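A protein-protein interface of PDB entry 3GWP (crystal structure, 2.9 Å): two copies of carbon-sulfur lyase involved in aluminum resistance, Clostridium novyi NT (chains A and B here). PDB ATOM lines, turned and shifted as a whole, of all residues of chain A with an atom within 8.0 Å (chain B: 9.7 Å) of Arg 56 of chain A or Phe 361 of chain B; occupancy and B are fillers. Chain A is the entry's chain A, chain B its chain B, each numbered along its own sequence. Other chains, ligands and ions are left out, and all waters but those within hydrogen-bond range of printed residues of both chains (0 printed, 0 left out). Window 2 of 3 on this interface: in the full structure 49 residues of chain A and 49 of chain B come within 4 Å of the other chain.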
ATOM      1  N   LEU A  49       5.879  26.693  29.834  1.00  0.00           N
ATOM      2  CA  LEU A  49       5.311  25.939  28.693  1.00  0.00           C
ATOM      3  C   LEU A  49       5.747  24.478  28.730  1.00  0.00           C
ATOM      4  O   LEU A  49       4.932  23.578  28.517  1.00  0.00           O
ATOM      5  CB  LEU A  49       5.720  26.585  27.350  1.00  0.00           C
ATOM      6  CG  LEU A  49       5.308  25.870  26.044  1.00  0.00           C
ATOM      7  CD1 LEU A  49       3.821  25.561  26.015  1.00  0.00           C
ATOM      8  CD2 LEU A  49       5.703  26.700  24.836  1.00  0.00           C
ATOM      9  N   ASN A  50       7.033  24.257  29.010  1.00  0.00           N
ATOM     10  CA  ASN A  50       7.589  22.914  29.116  1.00  0.00           C
ATOM     11  C   ASN A  50       6.938  22.119  30.259  1.00  0.00           C
ATOM     12  O   ASN A  50       6.575  20.965  30.076  1.00  0.00           O
ATOM     13  CB  ASN A  50       9.098  22.989  29.337  1.00  0.00           C
ATOM     14  CG  ASN A  50       9.746  21.630  29.409  1.00  0.00           C
ATOM     15  OD1 ASN A  50      10.386  21.296  30.400  1.00  0.00           O
ATOM     16  ND2 ASN A  50       9.530  20.811  28.387  1.00  0.00           N
ATOM     17  N   ALA A  51       6.782  22.763  31.422  1.00  0.00           N
ATOM     18  CA  ALA A  51       6.164  22.132  32.605  1.00  0.00           C
ATOM     19  C   ALA A  51       4.796  21.542  32.272  1.00  0.00           C
ATOM     20  O   ALA A  51       4.498  20.407  32.649  1.00  0.00           O
ATOM     21  CB  ALA A  51       6.042  23.136  33.731  1.00  0.00           C
ATOM     22  N   PHE A  52       3.966  22.326  31.579  1.00  0.00           N
ATOM     23  CA  PHE A  52       2.645  21.860  31.124  1.00  0.00           C
ATOM     24  C   PHE A  52       2.796  20.648  30.226  1.00  0.00           C
ATOM     25  O   PHE A  52       2.123  19.633  30.407  1.00  0.00           O
ATOM     26  CB  PHE A  52       1.911  22.961  30.336  1.00  0.00           C
ATOM     27  CG  PHE A  52       1.188  23.964  31.196  1.00  0.00           C
ATOM     28  CD1 PHE A  52       1.882  24.955  31.877  1.00  0.00           C
ATOM     29  CD2 PHE A  52      -0.204  23.962  31.261  1.00  0.00           C
ATOM     30  CE1 PHE A  52       1.212  25.890  32.648  1.00  0.00           C
ATOM     31  CE2 PHE A  52      -0.876  24.899  32.023  1.00  0.00           C
ATOM     32  CZ  PHE A  52      -0.164  25.862  32.719  1.00  0.00           C
ATOM     33  N   GLN A  53       3.703  20.763  29.264  1.00  0.00           N
ATOM     34  CA  GLN A  53       3.952  19.701  28.289  1.00  0.00           C
ATOM     35  C   GLN A  53       4.537  18.429  28.924  1.00  0.00           C
ATOM     36  O   GLN A  53       4.107  17.324  28.592  1.00  0.00           O
ATOM     37  CB  GLN A  53       4.842  20.233  27.154  1.00  0.00           C
ATOM     38  CG  GLN A  53       4.132  21.311  26.291  1.00  0.00           C
ATOM     39  CD  GLN A  53       5.058  22.033  25.330  1.00  0.00           C
ATOM     40  OE1 GLN A  53       6.278  21.965  25.452  1.00  0.00           O
ATOM     41  NE2 GLN A  53       4.471  22.764  24.386  1.00  0.00           N
ATOM     42  N   GLU A  54       5.487  18.589  29.849  1.00  0.00           N
ATOM     43  CA  GLU A  54       6.080  17.441  30.554  1.00  0.00           C
ATOM     44  C   GLU A  54       5.008  16.710  31.360  1.00  0.00           C
ATOM     45  O   GLU A  54       4.970  15.483  31.373  1.00  0.00           O
ATOM     46  CB  GLU A  54       7.217  17.886  31.494  1.00  0.00           C
ATOM     47  CG  GLU A  54       8.488  18.433  30.797  1.00  0.00           C
ATOM     48  CD  GLU A  54       9.380  17.353  30.195  1.00  0.00           C
ATOM     49  OE1 GLU A  54       8.910  16.221  29.958  1.00  0.00           O
ATOM     50  OE2 GLU A  54      10.563  17.654  29.949  1.00  0.00           O
ATOM     51  N   GLU A  55       4.136  17.477  32.027  1.00  0.00           N
ATOM     52  CA  GLU A  55       3.020  16.895  32.797  1.00  0.00           C
ATOM     53  C   GLU A  55       1.845  16.406  31.932  1.00  0.00           C
ATOM     54  O   GLU A  55       0.888  15.835  32.460  1.00  0.00           O
ATOM     55  CB  GLU A  55       2.540  17.839  33.913  1.00  0.00           C
ATOM     56  CG  GLU A  55       3.333  17.678  35.195  1.00  0.00           C
ATOM     57  CD  GLU A  55       3.163  16.279  35.814  1.00  0.00           C
ATOM     58  OE1 GLU A  55       2.060  15.700  35.706  1.00  0.00           O
ATOM     59  OE2 GLU A  55       4.125  15.771  36.417  1.00  0.00           O
ATOM     60  N   ARG A  56       1.905  16.673  30.622  1.00  0.00           N
ATOM     61  CA  ARG A  56       0.939  16.145  29.671  1.00  0.00           C
ATOM     62  C   ARG A  56      -0.488  16.668  29.967  1.00  0.00           C
ATOM     63  O   ARG A  56      -1.475  15.924  29.905  1.00  0.00           O
ATOM     64  CB  ARG A  56       1.036  14.600  29.708  1.00  0.00           C
ATOM     65  CG  ARG A  56       0.680  13.905  28.444  1.00  0.00           C
ATOM     66  CD  ARG A  56       1.168  12.452  28.439  1.00  0.00           C
ATOM     67  NE  ARG A  56       1.036  11.858  27.109  1.00  0.00           N
ATOM     68  CZ  ARG A  56       1.503  10.659  26.755  1.00  0.00           C
ATOM     69  NH1 ARG A  56       2.123   9.864  27.639  1.00  0.00           N
ATOM     70  NH2 ARG A  56       1.330  10.235  25.498  1.00  0.00           N
ATOM     71  N   ILE A  57      -0.558  17.976  30.243  1.00  0.00           N
ATOM     72  CA  ILE A  57      -1.809  18.675  30.589  1.00  0.00           C
ATOM     73  C   ILE A  57      -2.777  18.690  29.409  1.00  0.00           C
ATOM     74  O   ILE A  57      -2.358  18.816  28.258  1.00  0.00           O
ATOM     75  CB  ILE A  57      -1.517  20.140  31.056  1.00  0.00           C
ATOM     76  CG1 ILE A  57      -0.662  20.152  32.335  1.00  0.00           C
ATOM     77  CG2 ILE A  57      -2.793  20.898  31.309  1.00  0.00           C
ATOM     78  CD1 ILE A  57      -1.310  19.492  33.524  1.00  0.00           C
ATOM     79  N   SER A  58      -4.074  18.620  29.719  1.00  0.00           N
ATOM     80  CA  SER A  58      -5.131  18.528  28.713  1.00  0.00           C
ATOM     81  C   SER A  58      -6.441  19.150  29.195  1.00  0.00           C
ATOM     82  O   SER A  58      -6.533  19.654  30.320  1.00  0.00           O
ATOM     83  CB  SER A  58      -5.383  17.049  28.398  1.00  0.00           C
ATOM     84  OG  SER A  58      -5.775  16.343  29.567  1.00  0.00           O
ATOM     85  N   GLU A  59      -7.444  19.134  28.315  1.00  0.00           N
ATOM     86  CA  GLU A  59      -8.800  19.609  28.658  1.00  0.00           C
ATOM     87  C   GLU A  59      -9.426  18.850  29.853  1.00  0.00           C
ATOM     88  O   GLU A  59     -10.287  19.390  30.542  1.00  0.00           O
ATOM     89  CB  GLU A  59      -9.769  19.622  27.419  1.00  0.00           C
ATOM     90  CG  GLU A  59      -9.540  18.540  26.257  1.00  0.00           C
ATOM     91  CD  GLU A  59      -9.429  17.059  26.726  1.00  0.00           C
ATOM     92  OE1 GLU A  59     -10.013  16.691  27.767  1.00  0.00           O
ATOM     93  OE2 GLU A  59      -8.789  16.256  25.997  1.00  0.00           O
ATOM     94  N   ALA A  60      -8.978  17.609  30.092  1.00  0.00           N
ATOM     95  CA  ALA A  60      -9.473  16.796  31.215  1.00  0.00           C
ATOM     96  C   ALA A  60      -8.960  17.292  32.591  1.00  0.00           C
ATOM     97  O   ALA A  60      -9.544  16.959  33.631  1.00  0.00           O
ATOM     98  CB  ALA A  60      -9.099  15.333  31.008  1.00  0.00           C
ATOM     99  N   HIS A  61      -7.874  18.077  32.591  1.00  0.00           N
ATOM    100  CA  HIS A  61      -7.297  18.621  33.841  1.00  0.00           C
ATOM    101  C   HIS A  61      -8.031  19.866  34.381  1.00  0.00           C
ATOM    102  O   HIS A  61      -7.693  20.360  35.459  1.00  0.00           O
ATOM    103  CB  HIS A  61      -5.800  18.916  33.661  1.00  0.00           C
ATOM    104  CG  HIS A  61      -4.966  17.686  33.500  1.00  0.00           C
ATOM    105  ND1 HIS A  61      -4.713  17.112  32.275  1.00  0.00           N
ATOM    106  CD2 HIS A  61      -4.367  16.893  34.417  1.00  0.00           C
ATOM    107  CE1 HIS A  61      -3.971  16.034  32.440  1.00  0.00           C
ATOM    108  NE2 HIS A  61      -3.750  15.877  33.732  1.00  0.00           N
ATOM    109  N   SER A  77      -2.006  17.461  39.100  1.00  0.00           N
ATOM    110  CA  SER A  77      -1.146  17.853  37.976  1.00  0.00           C
ATOM    111  C   SER A  77      -0.730  19.323  38.071  1.00  0.00           C
ATOM    112  O   SER A  77       0.310  19.698  37.537  1.00  0.00           O
ATOM    113  CB  SER A  77      -1.816  17.576  36.637  1.00  0.00           C
ATOM    114  OG  SER A  77      -1.922  16.187  36.409  1.00  0.00           O
ATOM    115  N   VAL A  81       3.036  20.502  38.011  1.00  0.00           N
ATOM    116  CA  VAL A  81       3.488  21.525  37.062  1.00  0.00           C
ATOM    117  C   VAL A  81       4.338  22.564  37.800  1.00  0.00           C
ATOM    118  O   VAL A  81       5.427  22.915  37.337  1.00  0.00           O
ATOM    119  CB  VAL A  81       2.309  22.202  36.324  1.00  0.00           C
ATOM    120  CG1 VAL A  81       2.770  23.472  35.620  1.00  0.00           C
ATOM    121  CG2 VAL A  81       1.681  21.231  35.331  1.00  0.00           C
ATOM    122  N   ARG A  84       7.768  21.236  38.642  1.00  0.00           N
ATOM    123  CA  ARG A  84       8.662  21.291  37.470  1.00  0.00           C
ATOM    124  C   ARG A  84       9.135  22.712  37.170  1.00  0.00           C
ATOM    125  O   ARG A  84      10.261  22.899  36.689  1.00  0.00           O
ATOM    126  CB  ARG A  84       7.990  20.700  36.233  1.00  0.00           C
ATOM    127  CG  ARG A  84       7.826  19.214  36.294  1.00  0.00           C
ATOM    128  CD  ARG A  84       7.138  18.696  35.073  1.00  0.00           C
ATOM    129  NE  ARG A  84       6.926  17.256  35.157  1.00  0.00           N
ATOM    130  CZ  ARG A  84       7.835  16.331  34.852  1.00  0.00           C
ATOM    131  NH1 ARG A  84       9.083  16.665  34.489  1.00  0.00           N
ATOM    132  NH2 ARG A  84       7.510  15.049  34.962  1.00  0.00           N
ATOM    133  N   LYS B 350       1.607  20.077  13.167  1.00  0.00           N
ATOM    134  CA  LYS B 350       2.067  19.179  14.248  1.00  0.00           C
ATOM    135  C   LYS B 350       3.042  19.913  15.181  1.00  0.00           C
ATOM    136  O   LYS B 350       3.031  19.703  16.397  1.00  0.00           O
ATOM    137  CB  LYS B 350       2.742  17.929  13.674  1.00  0.00           C
ATOM    138  CG  LYS B 350       1.797  16.937  13.014  1.00  0.00           C
ATOM    139  CD  LYS B 350       2.568  15.774  12.403  1.00  0.00           C
ATOM    140  CE  LYS B 350       1.651  14.671  11.896  1.00  0.00           C
ATOM    141  NZ  LYS B 350       0.916  14.000  13.000  1.00  0.00           N
ATOM    142  N   ILE B 352       3.057  23.217  15.702  1.00  0.00           N
ATOM    143  CA  ILE B 352       2.273  24.192  16.476  1.00  0.00           C
ATOM    144  C   ILE B 352       1.537  23.468  17.615  1.00  0.00           C
ATOM    145  O   ILE B 352       1.494  23.956  18.749  1.00  0.00           O
ATOM    146  CB  ILE B 352       1.239  24.970  15.585  1.00  0.00           C
ATOM    147  CG1 ILE B 352       1.952  25.841  14.538  1.00  0.00           C
ATOM    148  CG2 ILE B 352       0.332  25.848  16.444  1.00  0.00           C
ATOM    149  CD1 ILE B 352       2.816  26.959  15.124  1.00  0.00           C
ATOM    150  N   GLN B 353       0.982  22.298  17.307  1.00  0.00           N
ATOM    151  CA  GLN B 353       0.279  21.507  18.295  1.00  0.00           C
ATOM    152  C   GLN B 353       1.226  21.097  19.400  1.00  0.00           C
ATOM    153  O   GLN B 353       0.904  21.239  20.576  1.00  0.00           O
ATOM    154  CB  GLN B 353      -0.330  20.253  17.652  1.00  0.00           C
ATOM    155  CG  GLN B 353      -1.216  19.409  18.595  1.00  0.00           C
ATOM    156  CD  GLN B 353      -2.450  20.158  19.071  1.00  0.00           C
ATOM    157  OE1 GLN B 353      -2.932  21.067  18.407  1.00  0.00           O
ATOM    158  NE2 GLN B 353      -2.976  19.759  20.214  1.00  0.00           N
ATOM    159  N   THR B 354       2.417  20.630  19.016  1.00  0.00           N
ATOM    160  CA  THR B 354       3.424  20.176  19.983  1.00  0.00           C
ATOM    161  C   THR B 354       3.976  21.326  20.869  1.00  0.00           C
ATOM    162  O   THR B 354       4.508  21.070  21.946  1.00  0.00           O
ATOM    163  CB  THR B 354       4.589  19.410  19.279  1.00  0.00           C
ATOM    164  OG1 THR B 354       5.335  18.668  20.246  1.00  0.00           O
ATOM    165  CG2 THR B 354       5.499  20.345  18.555  1.00  0.00           C
ATOM    166  N   GLY B 355       3.827  22.577  20.411  1.00  0.00           N
ATOM    167  CA  GLY B 355       4.239  23.765  21.189  1.00  0.00           C
ATOM    168  C   GLY B 355       3.074  24.460  21.921  1.00  0.00           C
ATOM    169  O   GLY B 355       3.106  25.672  22.130  1.00  0.00           O
ATOM    170  N   SER B 356       2.052  23.690  22.308  1.00  0.00           N
ATOM    171  CA  SER B 356       0.876  24.230  23.007  1.00  0.00           C
ATOM    172  C   SER B 356       0.845  23.722  24.468  1.00  0.00           C
ATOM    173  O   SER B 356       1.300  22.614  24.742  1.00  0.00           O
ATOM    174  CB  SER B 356      -0.402  23.811  22.280  1.00  0.00           C
ATOM    175  OG  SER B 356      -0.385  24.241  20.924  1.00  0.00           O
ATOM    176  N   PRO B 357       0.297  24.538  25.407  1.00  0.00           N
ATOM    177  CA  PRO B 357       0.254  24.121  26.817  1.00  0.00           C
ATOM    178  C   PRO B 357      -0.727  22.961  27.080  1.00  0.00           C
ATOM    179  O   PRO B 357      -0.391  22.028  27.809  1.00  0.00           O
ATOM    180  CB  PRO B 357      -0.191  25.395  27.548  1.00  0.00           C
ATOM    181  CG  PRO B 357      -0.925  26.180  26.548  1.00  0.00           C
ATOM    182  CD  PRO B 357      -0.334  25.858  25.206  1.00  0.00           C
ATOM    183  N   ILE B 358      -1.906  23.021  26.461  1.00  0.00           N
ATOM    184  CA  ILE B 358      -2.927  21.991  26.612  1.00  0.00           C
ATOM    185  C   ILE B 358      -2.930  21.079  25.379  1.00  0.00           C
ATOM    186  O   ILE B 358      -2.827  21.561  24.252  1.00  0.00           O
ATOM    187  CB  ILE B 358      -4.342  22.624  26.766  1.00  0.00           C
ATOM    188  CG1 ILE B 358      -4.339  23.735  27.828  1.00  0.00           C
ATOM    189  CG2 ILE B 358      -5.372  21.562  27.103  1.00  0.00           C
ATOM    190  CD1 ILE B 358      -3.805  23.301  29.171  1.00  0.00           C
ATOM    191  N   ASP B 359      -3.018  19.766  25.608  1.00  0.00           N
ATOM    192  CA  ASP B 359      -3.072  18.755  24.520  1.00  0.00           C
ATOM    193  C   ASP B 359      -1.865  18.757  23.553  1.00  0.00           C
ATOM    194  O   ASP B 359      -2.038  18.635  22.343  1.00  0.00           O
ATOM    195  CB  ASP B 359      -4.395  18.890  23.728  1.00  0.00           C
ATOM    196  CG  ASP B 359      -5.616  18.625  24.584  1.00  0.00           C
ATOM    197  OD1 ASP B 359      -5.645  17.585  25.278  1.00  0.00           O
ATOM    198  OD2 ASP B 359      -6.576  19.425  24.514  1.00  0.00           O
ATOM    199  N   SER B 360      -0.653  18.876  24.096  1.00  0.00           N
ATOM    200  CA  SER B 360       0.571  18.850  23.266  1.00  0.00           C
ATOM    201  C   SER B 360       0.809  17.438  22.752  1.00  0.00           C
ATOM    202  O   SER B 360       1.127  17.234  21.588  1.00  0.00           O
ATOM    203  CB  SER B 360       1.783  19.322  24.068  1.00  0.00           C
ATOM    204  OG  SER B 360       1.963  18.554  25.249  1.00  0.00           O
ATOM    205  N   PHE B 361       0.682  16.482  23.660  1.00  0.00           N
ATOM    206  CA  PHE B 361       0.827  15.043  23.370  1.00  0.00           C
ATOM    207  C   PHE B 361      -0.139  14.487  22.296  1.00  0.00           C
ATOM    208  O   PHE B 361       0.179  13.506  21.637  1.00  0.00           O
ATOM    209  CB  PHE B 361       0.642  14.234  24.670  1.00  0.00           C
ATOM    210  CG  PHE B 361      -0.742  14.375  25.291  1.00  0.00           C
ATOM    211  CD1 PHE B 361      -1.028  15.414  26.173  1.00  0.00           C
ATOM    212  CD2 PHE B 361      -1.748  13.459  24.998  1.00  0.00           C
ATOM    213  CE1 PHE B 361      -2.272  15.534  26.742  1.00  0.00           C
ATOM    214  CE2 PHE B 361      -3.007  13.586  25.561  1.00  0.00           C
ATOM    215  CZ  PHE B 361      -3.268  14.623  26.434  1.00  0.00           C
ATOM    216  N   VAL B 362      -1.318  15.103  22.162  1.00  0.00           N
ATOM    217  CA  VAL B 362      -2.353  14.658  21.200  1.00  0.00           C
ATOM    218  C   VAL B 362      -1.851  14.533  19.741  1.00  0.00           C
ATOM    219  O   VAL B 362      -1.061  15.353  19.272  1.00  0.00           O
ATOM    220  CB  VAL B 362      -3.602  15.608  21.245  1.00  0.00           C
ATOM    221  CG1 VAL B 362      -4.562  15.312  20.097  1.00  0.00           C
ATOM    222  CG2 VAL B 362      -4.319  15.483  22.588  1.00  0.00           C
ATOM    223  N   SER B 363      -2.305  13.477  19.056  1.00  0.00           N
ATOM    224  CA  SER B 363      -1.938  13.222  17.662  1.00  0.00           C
ATOM    225  C   SER B 363      -2.601  14.234  16.726  1.00  0.00           C
ATOM    226  O   SER B 363      -3.824  14.389  16.747  1.00  0.00           O
ATOM    227  CB  SER B 363      -2.356  11.811  17.256  1.00  0.00           C
ATOM    228  OG  SER B 363      -2.086  11.576  15.885  1.00  0.00           O
ATOM    229  N   CYS B 364      -1.791  14.898  15.894  1.00  0.00           N
ATOM    230  CA  CYS B 364      -2.282  15.907  14.938  1.00  0.00           C
ATOM    231  C   CYS B 364      -2.223  15.393  13.487  1.00  0.00           C
ATOM    232  O   CYS B 364      -1.204  15.517  12.815  1.00  0.00           O
ATOM    233  CB  CYS B 364      -1.478  17.201  15.079  1.00  0.00           C
ATOM    234  SG  CYS B 364      -1.865  18.438  13.843  1.00  0.00           S
ATOM    235  N   GLU B 365      -3.335  14.815  13.031  1.00  0.00           N
ATOM    236  CA  GLU B 365      -3.464  14.271  11.680  1.00  0.00           C
ATOM    237  C   GLU B 365      -4.661  14.941  11.001  1.00  0.00           C
ATOM    238  O   GLU B 365      -5.439  15.630  11.668  1.00  0.00           O
ATOM    239  CB  GLU B 365      -3.715  12.756  11.744  1.00  0.00           C
ATOM    240  CG  GLU B 365      -2.642  11.936  12.486  1.00  0.00           C
ATOM    241  CD  GLU B 365      -1.289  11.904  11.778  1.00  0.00           C
ATOM    242  OE1 GLU B 365      -1.219  12.247  10.580  1.00  0.00           O
ATOM    243  OE2 GLU B 365      -0.296  11.493  12.420  1.00  0.00           O
ATOM    244  N   ALA B 380      -4.885  22.726  17.692  1.00  0.00           N
ATOM    245  CA  ALA B 380      -5.646  23.394  18.743  1.00  0.00           C
ATOM    246  C   ALA B 380      -5.280  22.830  20.117  1.00  0.00           C
ATOM    247  O   ALA B 380      -5.121  21.627  20.282  1.00  0.00           O
ATOM    248  CB  ALA B 380      -7.137  23.236  18.489  1.00  0.00           C
ATOM    249  N   GLY B 381      -5.158  23.708  21.096  1.00  0.00           N
ATOM    250  CA  GLY B 381      -4.811  23.307  22.444  1.00  0.00           C
ATOM    251  C   GLY B 381      -4.836  24.516  23.339  1.00  0.00           C
ATOM    252  O   GLY B 381      -3.792  25.091  23.638  1.00  0.00           O
ATOM    253  N   ARG B 424      10.888  21.966  12.275  1.00  0.00           N
ATOM    254  CA  ARG B 424      10.432  20.645  11.922  1.00  0.00           C
ATOM    255  C   ARG B 424      10.495  20.476  10.379  1.00  0.00           C
ATOM    256  O   ARG B 424      10.618  19.359   9.879  1.00  0.00           O
ATOM    257  CB  ARG B 424       9.005  20.463  12.470  1.00  0.00           C
ATOM    258  CG  ARG B 424       8.629  19.057  12.839  1.00  0.00           C
ATOM    259  CD  ARG B 424       7.435  19.050  13.814  1.00  0.00           C
ATOM    260  NE  ARG B 424       7.214  17.718  14.389  1.00  0.00           N
ATOM    261  CZ  ARG B 424       6.455  16.751  13.856  1.00  0.00           C
ATOM    262  NH1 ARG B 424       5.790  16.939  12.711  1.00  0.00           N
ATOM    263  NH2 ARG B 424       6.355  15.574  14.482  1.00  0.00           N
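Gly 355 of chain B touches Leu 49 of chain A.
Leu 49 of chain A touches Pro 357 of chain B (CD1 to N, 3.7 Å).
O of Pro 357 of chain B touches CB of Phe 52 of chain A, 3.5 Å away.
Gly 355 of chain B touches Gln 53 of chain A (C to NE2, 3.3 Å).
Ser 360 of chain B touches Gln 53 of chain A (OG to CG, 3.7 Å).
Arg 56 of chain A touches Phe 361 of chain B.
Ile 57 of chain A touches Ile 358 of chain B.
Ile 57 of chain A touches Phe 361 of chain B.
OD1 of Asp 359 of chain B touches CB of Ser 58 of chain A (3.2 Å).
Glu 59 of chain A touches Ile 358 of chain B.
Printed residues of chain B within 4 Å of Phe 52 of chain A: Pro 357 (3.5 Å).
Of the printed residues of chain B, Gln 53 of chain A touches Thr 354 (3.0 Å), Gly 355 (3.3 Å), Ser 356 (3.2 Å) and Ser 360 (3.7 Å).
Arg 56 of chain A touches just one residue of chain B: Phe 361 (3.2 Å).
Gln 353 of chain B touches none of the printed residues of chain A.
Printed residues of chain A within 4 Å of Ser 356 of chain B: Leu 49 and Gln 53.
Printed residues of chain A within 4 Å of Pro 357 of chain B: Leu 49, Phe 52 and Ile 57.
Of the printed residues of chain A, Asp 359 of chain B touches Ile 57, Ser 58 and Glu 59.
Of chain A, only Gln 53 (3.7 Å) comes within 4 Å of Ser 360 of chain B.
Of chain A, only Arg 56, Ile 57 and Ser 58 come within 4 Å of Phe 361 of chain B.
Arg 424 of chain B touches none of the printed residues of chain A.
The nearest printed residue of chain A that does not touch Gly 355 of chain B is Asn 50 of chain A (8.0 Å).
Of the 16 printed residues of chain A, 7 touch a printed residue of chain B.
Printed residues of chain A that touch a printed residue of chain B: Leu 49, Phe 52, Gln 53, Arg 56, Ile 57, Ser 58 and Glu 59.
Hydrophobic or aromatic side chains of chain A within 4 Å of the printed part of chain B: Leu 49, Phe 52 and Ile 57.
Hydrophobic or aromatic side chains of chain B within 4 Å of the printed part of chain A: Pro 357, Ile 358 and Phe 361.
Along chain B the printed residues that touch a printed residue of chain A span positions 354 to 361.
Among the printed residues, no Asp or Glu carboxylate lies within 4 Å of a Lys or Arg side-chain nitrogen of the other chain.
The backbone NH of Asp 359 of chain B lies within hydrogen-bond range of the backbone carbonyl oxygen of Ile 57 of chain A.
The side-chain amide nitrogen of Gln 53 of chain A lies within hydrogen-bond range of the backbone carbonyl oxygen of Ser 356 of chain B (3.2 Å).
OE2 of Glu 59 of chain A lies close to OD1 of Asp 359 of chain B, 3.5 Å away.
NE2 of Gln 53 of chain A sits at hydrogen-bond distance from O of Thr 354 of chain B, 3.0 Å away.
No position is printed for both chains.
Of the 18 pairs that touch across the chains among the printed residues, none has its exchanged pair printed and touching as well.
The backbone carbonyl oxygen (O) of Phe 52 of chain A sits at hydrogen-bond distance from the backbone NH (N) of Ile 57 of chain A, at 3.2 Å.
NE2 of Gln 353 of chain B is in hydrogen-bond range of O of Asp 359 of chain B (2.6 Å).
OG of Ser 58 of chain A lies close to N of Ala 60 of chain A (3.5 Å).
The side-chain hydroxyl of Ser 356 of chain B sits at hydrogen-bond distance from the backbone carbonyl oxygen of Gln 353 of chain B (3.3 Å).
The side-chain hydroxyl of Ser 356 of chain B lies within hydrogen-bond range of the backbone carbonyl oxygen of Ile 352 of chain B, at 2.9 Å.
The side-chain hydroxyl (OG) of Ser 58 of chain A sits at hydrogen-bond distance from a ring nitrogen (ND1) of His 61 of chain A.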
